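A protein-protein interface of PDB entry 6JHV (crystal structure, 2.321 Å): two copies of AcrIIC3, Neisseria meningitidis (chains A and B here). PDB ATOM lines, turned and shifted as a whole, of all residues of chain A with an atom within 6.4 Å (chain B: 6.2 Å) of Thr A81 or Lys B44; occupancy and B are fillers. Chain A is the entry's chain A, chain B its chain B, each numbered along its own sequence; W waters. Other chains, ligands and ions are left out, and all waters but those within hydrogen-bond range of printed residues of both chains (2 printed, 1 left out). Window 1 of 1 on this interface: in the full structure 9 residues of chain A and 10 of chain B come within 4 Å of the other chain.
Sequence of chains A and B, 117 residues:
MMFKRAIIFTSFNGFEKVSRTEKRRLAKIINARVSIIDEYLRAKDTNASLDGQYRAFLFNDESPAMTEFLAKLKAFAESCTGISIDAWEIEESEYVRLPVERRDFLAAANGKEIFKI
Water W2 bridges the side-chain carboxylate (OD1) of Asp B45 (2.4 Å) and the backbone carbonyl oxygen (O) of Thr A81 (3.0 Å).
Water W1 bridges the side-chain carboxylate (OD1) of Asp B45 and the side-chain amide nitrogen (ND2) of Asn A13.
No position is printed for both chains.
Of the 12 pairs that touch across the chains among the printed residues, none has its exchanged pair printed and touching as well.
The backbone carbonyl oxygen (O) of Ile A83 lies within hydrogen-bond range of the side-chain amino group (NZ) of Lys B44 (2.8 Å).
The backbone carbonyl oxygen (O) of Ser A79 sits close to the side-chain carboxylate (OE2) of Glu B39 (3.4 Å).
The backbone carbonyl oxygen (O) of Ala A77 sits at hydrogen-bond distance from the side-chain amino group (NZ) of Lys B44, 2.8 Å away.
The backbone carbonyl oxygen of Cys A80 is in hydrogen-bond range of the side-chain amino group of Lys B44 (3.5 Å).
Among the printed residues, merely in contact across the chains: Phe A15 with Asp B45, Phe A15 with Asn B31, Ile A117 with Lys B44, Phe A15 with Ala B27, Thr A81 with Lys B44, Phe A15 with Ala B43, Thr A81 with Ala B43 and Thr A81 with Arg B42.
The backbone NH (N) of Lys B44 sits at hydrogen-bond distance from the side-chain hydroxyl (OG) of Ser B49 (2.8 Å).
The side-chain amide oxygen of Asn B31 lies within hydrogen-bond range of the backbone NH of Ala B43 (2.8 Å).
The backbone carbonyl oxygen of Ile A85 sits at hydrogen-bond distance from the backbone NH of Ile A117.
SG of Cys A80 lies close to N of Gly A82, at 3.8 Å.
OE1 of Glu A22 sits close to SG of Cys A80 (3.5 Å).
N of Phe A15 is in hydrogen-bond range of OD1 of Asn A13 (2.7 Å).
Hydrophobic or aromatic side chains of chain A that line the printed part of chain B: Phe A15.
Among the printed residues, 12 pairs touch across the chains.
Thr A81 touches just these residues of chain B: Arg B42 (3.97 Å), Ala B43 (3.9 Å) and Lys B44 (3.8 Å).
Of chain A, only Ala A77, Cys A80, Thr A81, Ile A83 and Ile A117 come within 4 Å of Lys B44.
Of the printed residues of chain A, Glu B39 touches Ser A79 (3.4 Å).
Printed residues of chain B within 4 Å of Ile A117: Lys B44 (3.6 Å).
Of the printed residues of chain A, Asp B45 touches Phe A15.
Of the printed residues of chain B, Cys A80 touches Lys B44.
Ser A84 touches none of the printed residues of chain B.
The nearest printed residue of chain B that does not touch Cys A80 is Glu B39 (5.3 Å).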
ATOM      1  N   ASN A  13       4.690 -13.937 -11.269  1.00  0.00           N
ATOM      2  CA  ASN A  13       4.389 -12.767 -12.105  1.00  0.00           C
ATOM      3  C   ASN A  13       4.001 -13.115 -13.539  1.00  0.00           C
ATOM      4  O   ASN A  13       3.440 -12.259 -14.225  1.00  0.00           O
ATOM      5  CB  ASN A  13       5.586 -11.808 -12.133  1.00  0.00           C
ATOM      6  CG  ASN A  13       6.859 -12.489 -12.578  1.00  0.00           C
ATOM      7  OD1 ASN A  13       6.847 -13.317 -13.499  1.00  0.00           O
ATOM      8  ND2 ASN A  13       7.964 -12.173 -11.914  1.00  0.00           N
ATOM      9  N   GLY A  14       4.265 -14.346 -14.001  1.00  0.00           N
ATOM     10  CA  GLY A  14       3.894 -14.760 -15.344  1.00  0.00           C
ATOM     11  C   GLY A  14       4.945 -14.512 -16.414  1.00  0.00           C
ATOM     12  O   GLY A  14       4.748 -14.925 -17.568  1.00  0.00           O
ATOM     13  N   PHE A  15       6.052 -13.857 -16.069  1.00  0.00           N
ATOM     14  CA  PHE A  15       7.152 -13.674 -17.004  1.00  0.00           C
ATOM     15  C   PHE A  15       7.836 -14.995 -17.338  1.00  0.00           C
ATOM     16  O   PHE A  15       8.300 -15.191 -18.469  1.00  0.00           O
ATOM     17  CB  PHE A  15       8.164 -12.693 -16.418  1.00  0.00           C
ATOM     18  CG  PHE A  15       9.369 -12.465 -17.281  1.00  0.00           C
ATOM     19  CD1 PHE A  15       9.273 -11.722 -18.452  1.00  0.00           C
ATOM     20  CD2 PHE A  15      10.603 -12.979 -16.916  1.00  0.00           C
ATOM     21  CE1 PHE A  15      10.387 -11.507 -19.250  1.00  0.00           C
ATOM     22  CE2 PHE A  15      11.728 -12.762 -17.702  1.00  0.00           C
ATOM     23  CZ  PHE A  15      11.616 -12.024 -18.877  1.00  0.00           C
ATOM     24  N   GLU A  16       7.912 -15.903 -16.372  1.00  0.00           N
ATOM     25  CA  GLU A  16       8.685 -17.123 -16.508  1.00  0.00           C
ATOM     26  C   GLU A  16       8.028 -18.186 -15.646  1.00  0.00           C
ATOM     27  O   GLU A  16       7.411 -17.874 -14.621  1.00  0.00           O
ATOM     28  CB  GLU A  16      10.144 -16.895 -16.084  1.00  0.00           C
ATOM     29  CG  GLU A  16      11.054 -18.140 -16.138  1.00  0.00           C
ATOM     30  CD  GLU A  16      11.264 -18.686 -17.559  1.00  0.00           C
ATOM     31  OE1 GLU A  16      10.684 -19.747 -17.880  1.00  0.00           O
ATOM     32  OE2 GLU A  16      12.013 -18.072 -18.352  1.00  0.00           O
ATOM     33  N   LYS A  17       8.143 -19.441 -16.078  1.00  0.00           N
ATOM     34  CA  LYS A  17       7.645 -20.534 -15.259  1.00  0.00           C
ATOM     35  C   LYS A  17       8.457 -20.627 -13.971  1.00  0.00           C
ATOM     36  O   LYS A  17       9.662 -20.351 -13.943  1.00  0.00           O
ATOM     37  CB  LYS A  17       7.690 -21.867 -16.021  1.00  0.00           C
ATOM     38  CG  LYS A  17       7.058 -23.042 -15.250  1.00  0.00           C
ATOM     39  CD  LYS A  17       7.205 -24.386 -16.002  1.00  0.00           C
ATOM     40  CE  LYS A  17       6.621 -25.593 -15.217  1.00  0.00           C
ATOM     41  NZ  LYS A  17       5.963 -25.280 -13.896  1.00  0.00           N
ATOM     42  N   GLU A  22      12.479 -23.850  -7.256  1.00  0.00           N
ATOM     43  CA  GLU A  22      12.323 -22.448  -6.881  1.00  0.00           C
ATOM     44  C   GLU A  22      11.238 -22.293  -5.824  1.00  0.00           C
ATOM     45  O   GLU A  22      11.415 -21.546  -4.852  1.00  0.00           O
ATOM     46  CB  GLU A  22      12.022 -21.584  -8.113  1.00  0.00           C
ATOM     47  CG  GLU A  22      13.275 -21.037  -8.801  1.00  0.00           C
ATOM     48  CD  GLU A  22      13.031 -20.540 -10.232  1.00  0.00           C
ATOM     49  OE1 GLU A  22      13.942 -19.881 -10.798  1.00  0.00           O
ATOM     50  OE2 GLU A  22      11.938 -20.808 -10.792  1.00  0.00           O
ATOM     51  N   PHE A  76      16.676 -13.524  -3.251  1.00  0.00           N
ATOM     52  CA  PHE A  76      15.954 -14.568  -3.966  1.00  0.00           C
ATOM     53  C   PHE A  76      15.120 -13.988  -5.099  1.00  0.00           C
ATOM     54  O   PHE A  76      15.137 -14.506  -6.219  1.00  0.00           O
ATOM     55  CB  PHE A  76      15.046 -15.359  -3.028  1.00  0.00           C
ATOM     56  CG  PHE A  76      14.162 -16.327  -3.754  1.00  0.00           C
ATOM     57  CD1 PHE A  76      14.597 -17.623  -4.005  1.00  0.00           C
ATOM     58  CD2 PHE A  76      12.917 -15.937  -4.236  1.00  0.00           C
ATOM     59  CE1 PHE A  76      13.804 -18.516  -4.706  1.00  0.00           C
ATOM     60  CE2 PHE A  76      12.123 -16.814  -4.938  1.00  0.00           C
ATOM     61  CZ  PHE A  76      12.568 -18.123  -5.173  1.00  0.00           C
ATOM     62  N   ALA A  77      14.325 -12.954  -4.804  1.00  0.00           N
ATOM     63  CA  ALA A  77      13.462 -12.369  -5.826  1.00  0.00           C
ATOM     64  C   ALA A  77      14.267 -11.810  -6.998  1.00  0.00           C
ATOM     65  O   ALA A  77      13.803 -11.858  -8.143  1.00  0.00           O
ATOM     66  CB  ALA A  77      12.588 -11.270  -5.215  1.00  0.00           C
ATOM     67  N   GLU A  78      15.465 -11.279  -6.735  1.00  0.00           N
ATOM     68  CA  GLU A  78      16.286 -10.720  -7.805  1.00  0.00           C
ATOM     69  C   GLU A  78      16.778 -11.800  -8.760  1.00  0.00           C
ATOM     70  O   GLU A  78      16.844 -11.572  -9.967  1.00  0.00           O
ATOM     71  CB  GLU A  78      17.465  -9.953  -7.218  1.00  0.00           C
ATOM     72  CG  GLU A  78      17.164  -8.506  -6.913  1.00  0.00           C
ATOM     73  CD  GLU A  78      18.272  -7.855  -6.122  1.00  0.00           C
ATOM     74  OE1 GLU A  78      19.280  -8.552  -5.874  1.00  0.00           O
ATOM     75  OE2 GLU A  78      18.131  -6.659  -5.748  1.00  0.00           O
ATOM     76  N   SER A  79      17.119 -12.981  -8.251  1.00  0.00           N
ATOM     77  CA  SER A  79      17.664 -14.030  -9.102  1.00  0.00           C
ATOM     78  C   SER A  79      16.595 -14.910  -9.745  1.00  0.00           C
ATOM     79  O   SER A  79      16.916 -15.673 -10.660  1.00  0.00           O
ATOM     80  CB  SER A  79      18.624 -14.919  -8.307  1.00  0.00           C
ATOM     81  OG  SER A  79      17.905 -15.716  -7.364  1.00  0.00           O
ATOM     82  N   CYS A  80      15.341 -14.833  -9.312  1.00  0.00           N
ATOM     83  CA  CYS A  80      14.288 -15.693  -9.844  1.00  0.00           C
ATOM     84  C   CYS A  80      13.327 -14.842 -10.666  1.00  0.00           C
ATOM     85  O   CYS A  80      12.509 -14.101 -10.103  1.00  0.00           O
ATOM     86  CB  CYS A  80      13.560 -16.410  -8.713  1.00  0.00           C
ATOM     87  SG  CYS A  80      12.097 -17.291  -9.265  1.00  0.00           S
ATOM     88  N   THR A  81      13.420 -14.947 -11.992  1.00  0.00           N
ATOM     89  CA  THR A  81      12.639 -14.063 -12.857  1.00  0.00           C
ATOM     90  C   THR A  81      11.130 -14.286 -12.746  1.00  0.00           C
ATOM     91  O   THR A  81      10.360 -13.410 -13.149  1.00  0.00           O
ATOM     92  CB  THR A  81      13.070 -14.242 -14.321  1.00  0.00           C
ATOM     93  OG1 THR A  81      12.831 -15.591 -14.723  1.00  0.00           O
ATOM     94  CG2 THR A  81      14.559 -13.921 -14.507  1.00  0.00           C
ATOM     95  N   GLY A  82      10.681 -15.433 -12.212  1.00  0.00           N
ATOM     96  CA  GLY A  82       9.267 -15.753 -12.248  1.00  0.00           C
ATOM     97  C   GLY A  82       8.481 -15.344 -11.035  1.00  0.00           C
ATOM     98  O   GLY A  82       7.245 -15.435 -11.027  1.00  0.00           O
ATOM     99  N   ILE A  83       9.172 -14.887 -10.000  1.00  0.00           N
ATOM    100  CA  ILE A  83       8.570 -14.611  -8.702  1.00  0.00           C
ATOM    101  C   ILE A  83       8.764 -13.142  -8.364  1.00  0.00           C
ATOM    102  O   ILE A  83       9.860 -12.598  -8.538  1.00  0.00           O
ATOM    103  CB  ILE A  83       9.173 -15.507  -7.610  1.00  0.00           C
ATOM    104  CG1 ILE A  83       8.878 -16.981  -7.941  1.00  0.00           C
ATOM    105  CG2 ILE A  83       8.622 -15.095  -6.240  1.00  0.00           C
ATOM    106  CD1 ILE A  83       9.382 -17.990  -6.903  1.00  0.00           C
ATOM    107  N   SER A  84       7.697 -12.498  -7.915  1.00  0.00           N
ATOM    108  CA  SER A  84       7.759 -11.135  -7.398  1.00  0.00           C
ATOM    109  C   SER A  84       7.562 -11.164  -5.894  1.00  0.00           C
ATOM    110  O   SER A  84       6.747 -11.945  -5.384  1.00  0.00           O
ATOM    111  CB  SER A  84       6.684 -10.243  -8.021  1.00  0.00           C
ATOM    112  OG  SER A  84       6.736 -10.306  -9.431  1.00  0.00           O
ATOM    113  N   ILE A  85       8.288 -10.300  -5.189  1.00  0.00           N
ATOM    114  CA  ILE A  85       8.118 -10.155  -3.751  1.00  0.00           C
ATOM    115  C   ILE A  85       8.032  -8.678  -3.411  1.00  0.00           C
ATOM    116  O   ILE A  85       8.979  -7.925  -3.667  1.00  0.00           O
ATOM    117  CB  ILE A  85       9.247 -10.820  -2.943  1.00  0.00           C
ATOM    118  CG1 ILE A  85       9.503 -12.266  -3.406  1.00  0.00           C
ATOM    119  CG2 ILE A  85       8.924 -10.746  -1.460  1.00  0.00           C
ATOM    120  CD1 ILE A  85      10.267 -13.134  -2.394  1.00  0.00           C
ATOM    121  N   ILE A 117      10.385  -6.299  -5.761  1.00  0.00           N
ATOM    122  CA  ILE A 117      11.387  -6.862  -6.679  1.00  0.00           C
ATOM    123  C   ILE A 117      10.758  -7.855  -7.651  1.00  0.00           C
ATOM    124  O   ILE A 117       9.727  -8.451  -7.339  1.00  0.00           O
ATOM    125  CB  ILE A 117      12.532  -7.542  -5.921  1.00  0.00           C
ATOM    126  CG1 ILE A 117      13.162  -6.586  -4.910  1.00  0.00           C
ATOM    127  CG2 ILE A 117      13.580  -8.070  -6.914  1.00  0.00           C
ATOM    128  CD1 ILE A 117      13.703  -5.334  -5.533  1.00  0.00           C
ATOM    129  N   LYS B  23       7.613  -4.207 -21.406  1.00  0.00           N
ATOM    130  CA  LYS B  23       8.593  -4.665 -20.421  1.00  0.00           C
ATOM    131  C   LYS B  23       8.950  -6.134 -20.634  1.00  0.00           C
ATOM    132  O   LYS B  23      10.123  -6.517 -20.542  1.00  0.00           O
ATOM    133  CB  LYS B  23       8.080  -4.450 -18.991  1.00  0.00           C
ATOM    134  CG  LYS B  23       8.033  -3.002 -18.492  1.00  0.00           C
ATOM    135  CD  LYS B  23       7.375  -2.936 -17.088  1.00  0.00           C
ATOM    136  CE  LYS B  23       6.616  -1.615 -16.911  1.00  0.00           C
ATOM    137  NZ  LYS B  23       5.894  -1.524 -15.607  1.00  0.00           N
ATOM    138  N   ALA B  27      12.767  -7.450 -21.686  1.00  0.00           N
ATOM    139  CA  ALA B  27      13.475  -8.410 -20.841  1.00  0.00           C
ATOM    140  C   ALA B  27      13.720  -9.735 -21.571  1.00  0.00           C
ATOM    141  O   ALA B  27      14.731 -10.386 -21.316  1.00  0.00           O
ATOM    142  CB  ALA B  27      12.723  -8.639 -19.520  1.00  0.00           C
ATOM    143  N   ASN B  31      17.349 -11.462 -22.300  1.00  0.00           N
ATOM    144  CA  ASN B  31      17.597 -12.792 -21.781  1.00  0.00           C
ATOM    145  C   ASN B  31      17.886 -13.817 -22.875  1.00  0.00           C
ATOM    146  O   ASN B  31      18.412 -14.885 -22.565  1.00  0.00           O
ATOM    147  CB  ASN B  31      16.416 -13.226 -20.910  1.00  0.00           C
ATOM    148  CG  ASN B  31      16.322 -12.404 -19.621  1.00  0.00           C
ATOM    149  OD1 ASN B  31      17.263 -11.700 -19.250  1.00  0.00           O
ATOM    150  ND2 ASN B  31      15.189 -12.487 -18.948  1.00  0.00           N
ATOM    151  N   GLU B  39      24.609 -14.813 -15.431  1.00  0.00           N
ATOM    152  CA  GLU B  39      23.254 -14.593 -14.943  1.00  0.00           C
ATOM    153  C   GLU B  39      23.065 -13.191 -14.371  1.00  0.00           C
ATOM    154  O   GLU B  39      21.935 -12.696 -14.333  1.00  0.00           O
ATOM    155  CB  GLU B  39      22.895 -15.641 -13.882  1.00  0.00           C
ATOM    156  CG  GLU B  39      21.391 -15.806 -13.681  1.00  0.00           C
ATOM    157  CD  GLU B  39      20.876 -15.146 -12.389  1.00  0.00           C
ATOM    158  OE1 GLU B  39      21.664 -15.004 -11.418  1.00  0.00           O
ATOM    159  OE2 GLU B  39      19.683 -14.744 -12.358  1.00  0.00           O
ATOM    160  N   ARG B  42      20.935 -10.814 -16.320  1.00  0.00           N
ATOM    161  CA  ARG B  42      19.549 -11.191 -16.579  1.00  0.00           C
ATOM    162  C   ARG B  42      18.604 -10.034 -16.283  1.00  0.00           C
ATOM    163  O   ARG B  42      18.874  -9.178 -15.435  1.00  0.00           O
ATOM    164  CB  ARG B  42      19.162 -12.406 -15.723  1.00  0.00           C
ATOM    165  CG  ARG B  42      18.039 -13.259 -16.308  1.00  0.00           C
ATOM    166  CD  ARG B  42      18.409 -14.748 -16.316  1.00  0.00           C
ATOM    167  NE  ARG B  42      17.732 -15.521 -17.366  1.00  0.00           N
ATOM    168  CZ  ARG B  42      18.237 -15.798 -18.574  1.00  0.00           C
ATOM    169  NH1 ARG B  42      19.450 -15.375 -18.926  1.00  0.00           N
ATOM    170  NH2 ARG B  42      17.526 -16.510 -19.439  1.00  0.00           N
ATOM    171  N   ALA B  43      17.469 -10.029 -16.975  1.00  0.00           N
ATOM    172  CA  ALA B  43      16.462  -8.986 -16.811  1.00  0.00           C
ATOM    173  C   ALA B  43      15.137  -9.570 -16.334  1.00  0.00           C
ATOM    174  O   ALA B  43      14.783 -10.709 -16.650  1.00  0.00           O
ATOM    175  CB  ALA B  43      16.226  -8.209 -18.115  1.00  0.00           C
ATOM    176  N   LYS B  44      14.412  -8.772 -15.560  1.00  0.00           N
ATOM    177  CA  LYS B  44      13.014  -9.019 -15.250  1.00  0.00           C
ATOM    178  C   LYS B  44      12.171  -7.970 -15.961  1.00  0.00           C
ATOM    179  O   LYS B  44      12.657  -6.883 -16.316  1.00  0.00           O
ATOM    180  CB  LYS B  44      12.789  -8.998 -13.731  1.00  0.00           C
ATOM    181  CG  LYS B  44      13.529 -10.154 -12.992  1.00  0.00           C
ATOM    182  CD  LYS B  44      13.295 -10.175 -11.481  1.00  0.00           C
ATOM    183  CE  LYS B  44      11.882 -10.629 -11.106  1.00  0.00           C
ATOM    184  NZ  LYS B  44      11.705 -10.742  -9.610  1.00  0.00           N
ATOM    185  N   ASP B  45      10.908  -8.307 -16.202  1.00  0.00           N
ATOM    186  CA  ASP B  45      10.000  -7.361 -16.838  1.00  0.00           C
ATOM    187  C   ASP B  45       9.469  -6.324 -15.849  1.00  0.00           C
ATOM    188  O   ASP B  45       8.251  -6.148 -15.723  1.00  0.00           O
ATOM    189  CB  ASP B  45       8.843  -8.106 -17.517  1.00  0.00           C
ATOM    190  CG  ASP B  45       7.998  -8.940 -16.548  1.00  0.00           C
ATOM    191  OD1 ASP B  45       8.483  -9.310 -15.456  1.00  0.00           O
ATOM    192  OD2 ASP B  45       6.834  -9.243 -16.907  1.00  0.00           O
ATOM    193  N   THR B  46      10.374  -5.622 -15.159  1.00  0.00           N
ATOM    194  CA  THR B  46      10.012  -4.681 -14.109  1.00  0.00           C
ATOM    195  C   THR B  46      10.753  -3.360 -14.288  1.00  0.00           C
ATOM    196  O   THR B  46      11.823  -3.300 -14.907  1.00  0.00           O
ATOM    197  CB  THR B  46      10.342  -5.233 -12.714  1.00  0.00           C
ATOM    198  OG1 THR B  46      11.761  -5.339 -12.578  1.00  0.00           O
ATOM    199  CG2 THR B  46       9.698  -6.610 -12.486  1.00  0.00           C
ATOM    200  N   ASN B  47      10.180  -2.300 -13.701  1.00  0.00           N
ATOM    201  CA  ASN B  47      10.856  -1.006 -13.692  1.00  0.00           C
ATOM    202  C   ASN B  47      12.234  -1.108 -13.042  1.00  0.00           C
ATOM    203  O   ASN B  47      13.232  -0.623 -13.591  1.00  0.00           O
ATOM    204  CB  ASN B  47       9.999   0.038 -12.974  1.00  0.00           C
ATOM    205  CG  ASN B  47       8.698   0.330 -13.695  1.00  0.00           C
ATOM    206  OD1 ASN B  47       8.015  -0.576 -14.166  1.00  0.00           O
ATOM    207  ND2 ASN B  47       8.338   1.600 -13.758  1.00  0.00           N
ATOM    208  N   SER B  49      14.278  -3.592 -12.778  1.00  0.00           N
ATOM    209  CA  SER B  49      15.266  -4.303 -13.581  1.00  0.00           C
ATOM    210  C   SER B  49      15.657  -3.552 -14.856  1.00  0.00           C
ATOM    211  O   SER B  49      16.796  -3.688 -15.323  1.00  0.00           O
ATOM    212  CB  SER B  49      14.731  -5.685 -13.939  1.00  0.00           C
ATOM    213  OG  SER B  49      15.706  -6.429 -14.608  1.00  0.00           O
ATOM    214  N   LEU B  50      14.749  -2.746 -15.417  1.00  0.00           N
ATOM    215  CA  LEU B  50      14.917  -2.157 -16.742  1.00  0.00           C
ATOM    216  C   LEU B  50      15.121  -0.641 -16.783  1.00  0.00           C
ATOM    217  O   LEU B  50      15.790  -0.153 -17.696  1.00  0.00           O
ATOM    218  CB  LEU B  50      13.701  -2.490 -17.610  1.00  0.00           C
ATOM    219  CG  LEU B  50      13.379  -3.952 -17.869  1.00  0.00           C
ATOM    220  CD1 LEU B  50      12.035  -4.027 -18.527  1.00  0.00           C
ATOM    221  CD2 LEU B  50      14.442  -4.610 -18.745  1.00  0.00           C
ATOM    222  N   ARG B  55      23.865  -2.554 -18.857  1.00  0.00           N
ATOM    223  CA  ARG B  55      24.271  -3.944 -19.061  1.00  0.00           C
ATOM    224  C   ARG B  55      25.360  -3.973 -20.125  1.00  0.00           C
ATOM    225  O   ARG B  55      25.214  -3.351 -21.180  1.00  0.00           O
ATOM    226  CB  ARG B  55      23.084  -4.831 -19.485  1.00  0.00           C
ATOM    227  CG  ARG B  55      22.063  -5.110 -18.362  1.00  0.00           C
ATOM    228  CD  ARG B  55      20.779  -5.802 -18.862  1.00  0.00           C
ATOM    229  NE  ARG B  55      20.035  -6.312 -17.708  1.00  0.00           N
ATOM    230  CZ  ARG B  55      19.125  -5.622 -17.019  1.00  0.00           C
ATOM    231  NH1 ARG B  55      18.793  -4.387 -17.385  1.00  0.00           N
ATOM    232  NH2 ARG B  55      18.537  -6.172 -15.961  1.00  0.00           N
HETATM  233  O   HOH W   1       7.045  -9.004 -12.992  1.00  0.00           O
HETATM  234  O   HOH W   2      10.154 -10.730 -14.376  1.00  0.00           O
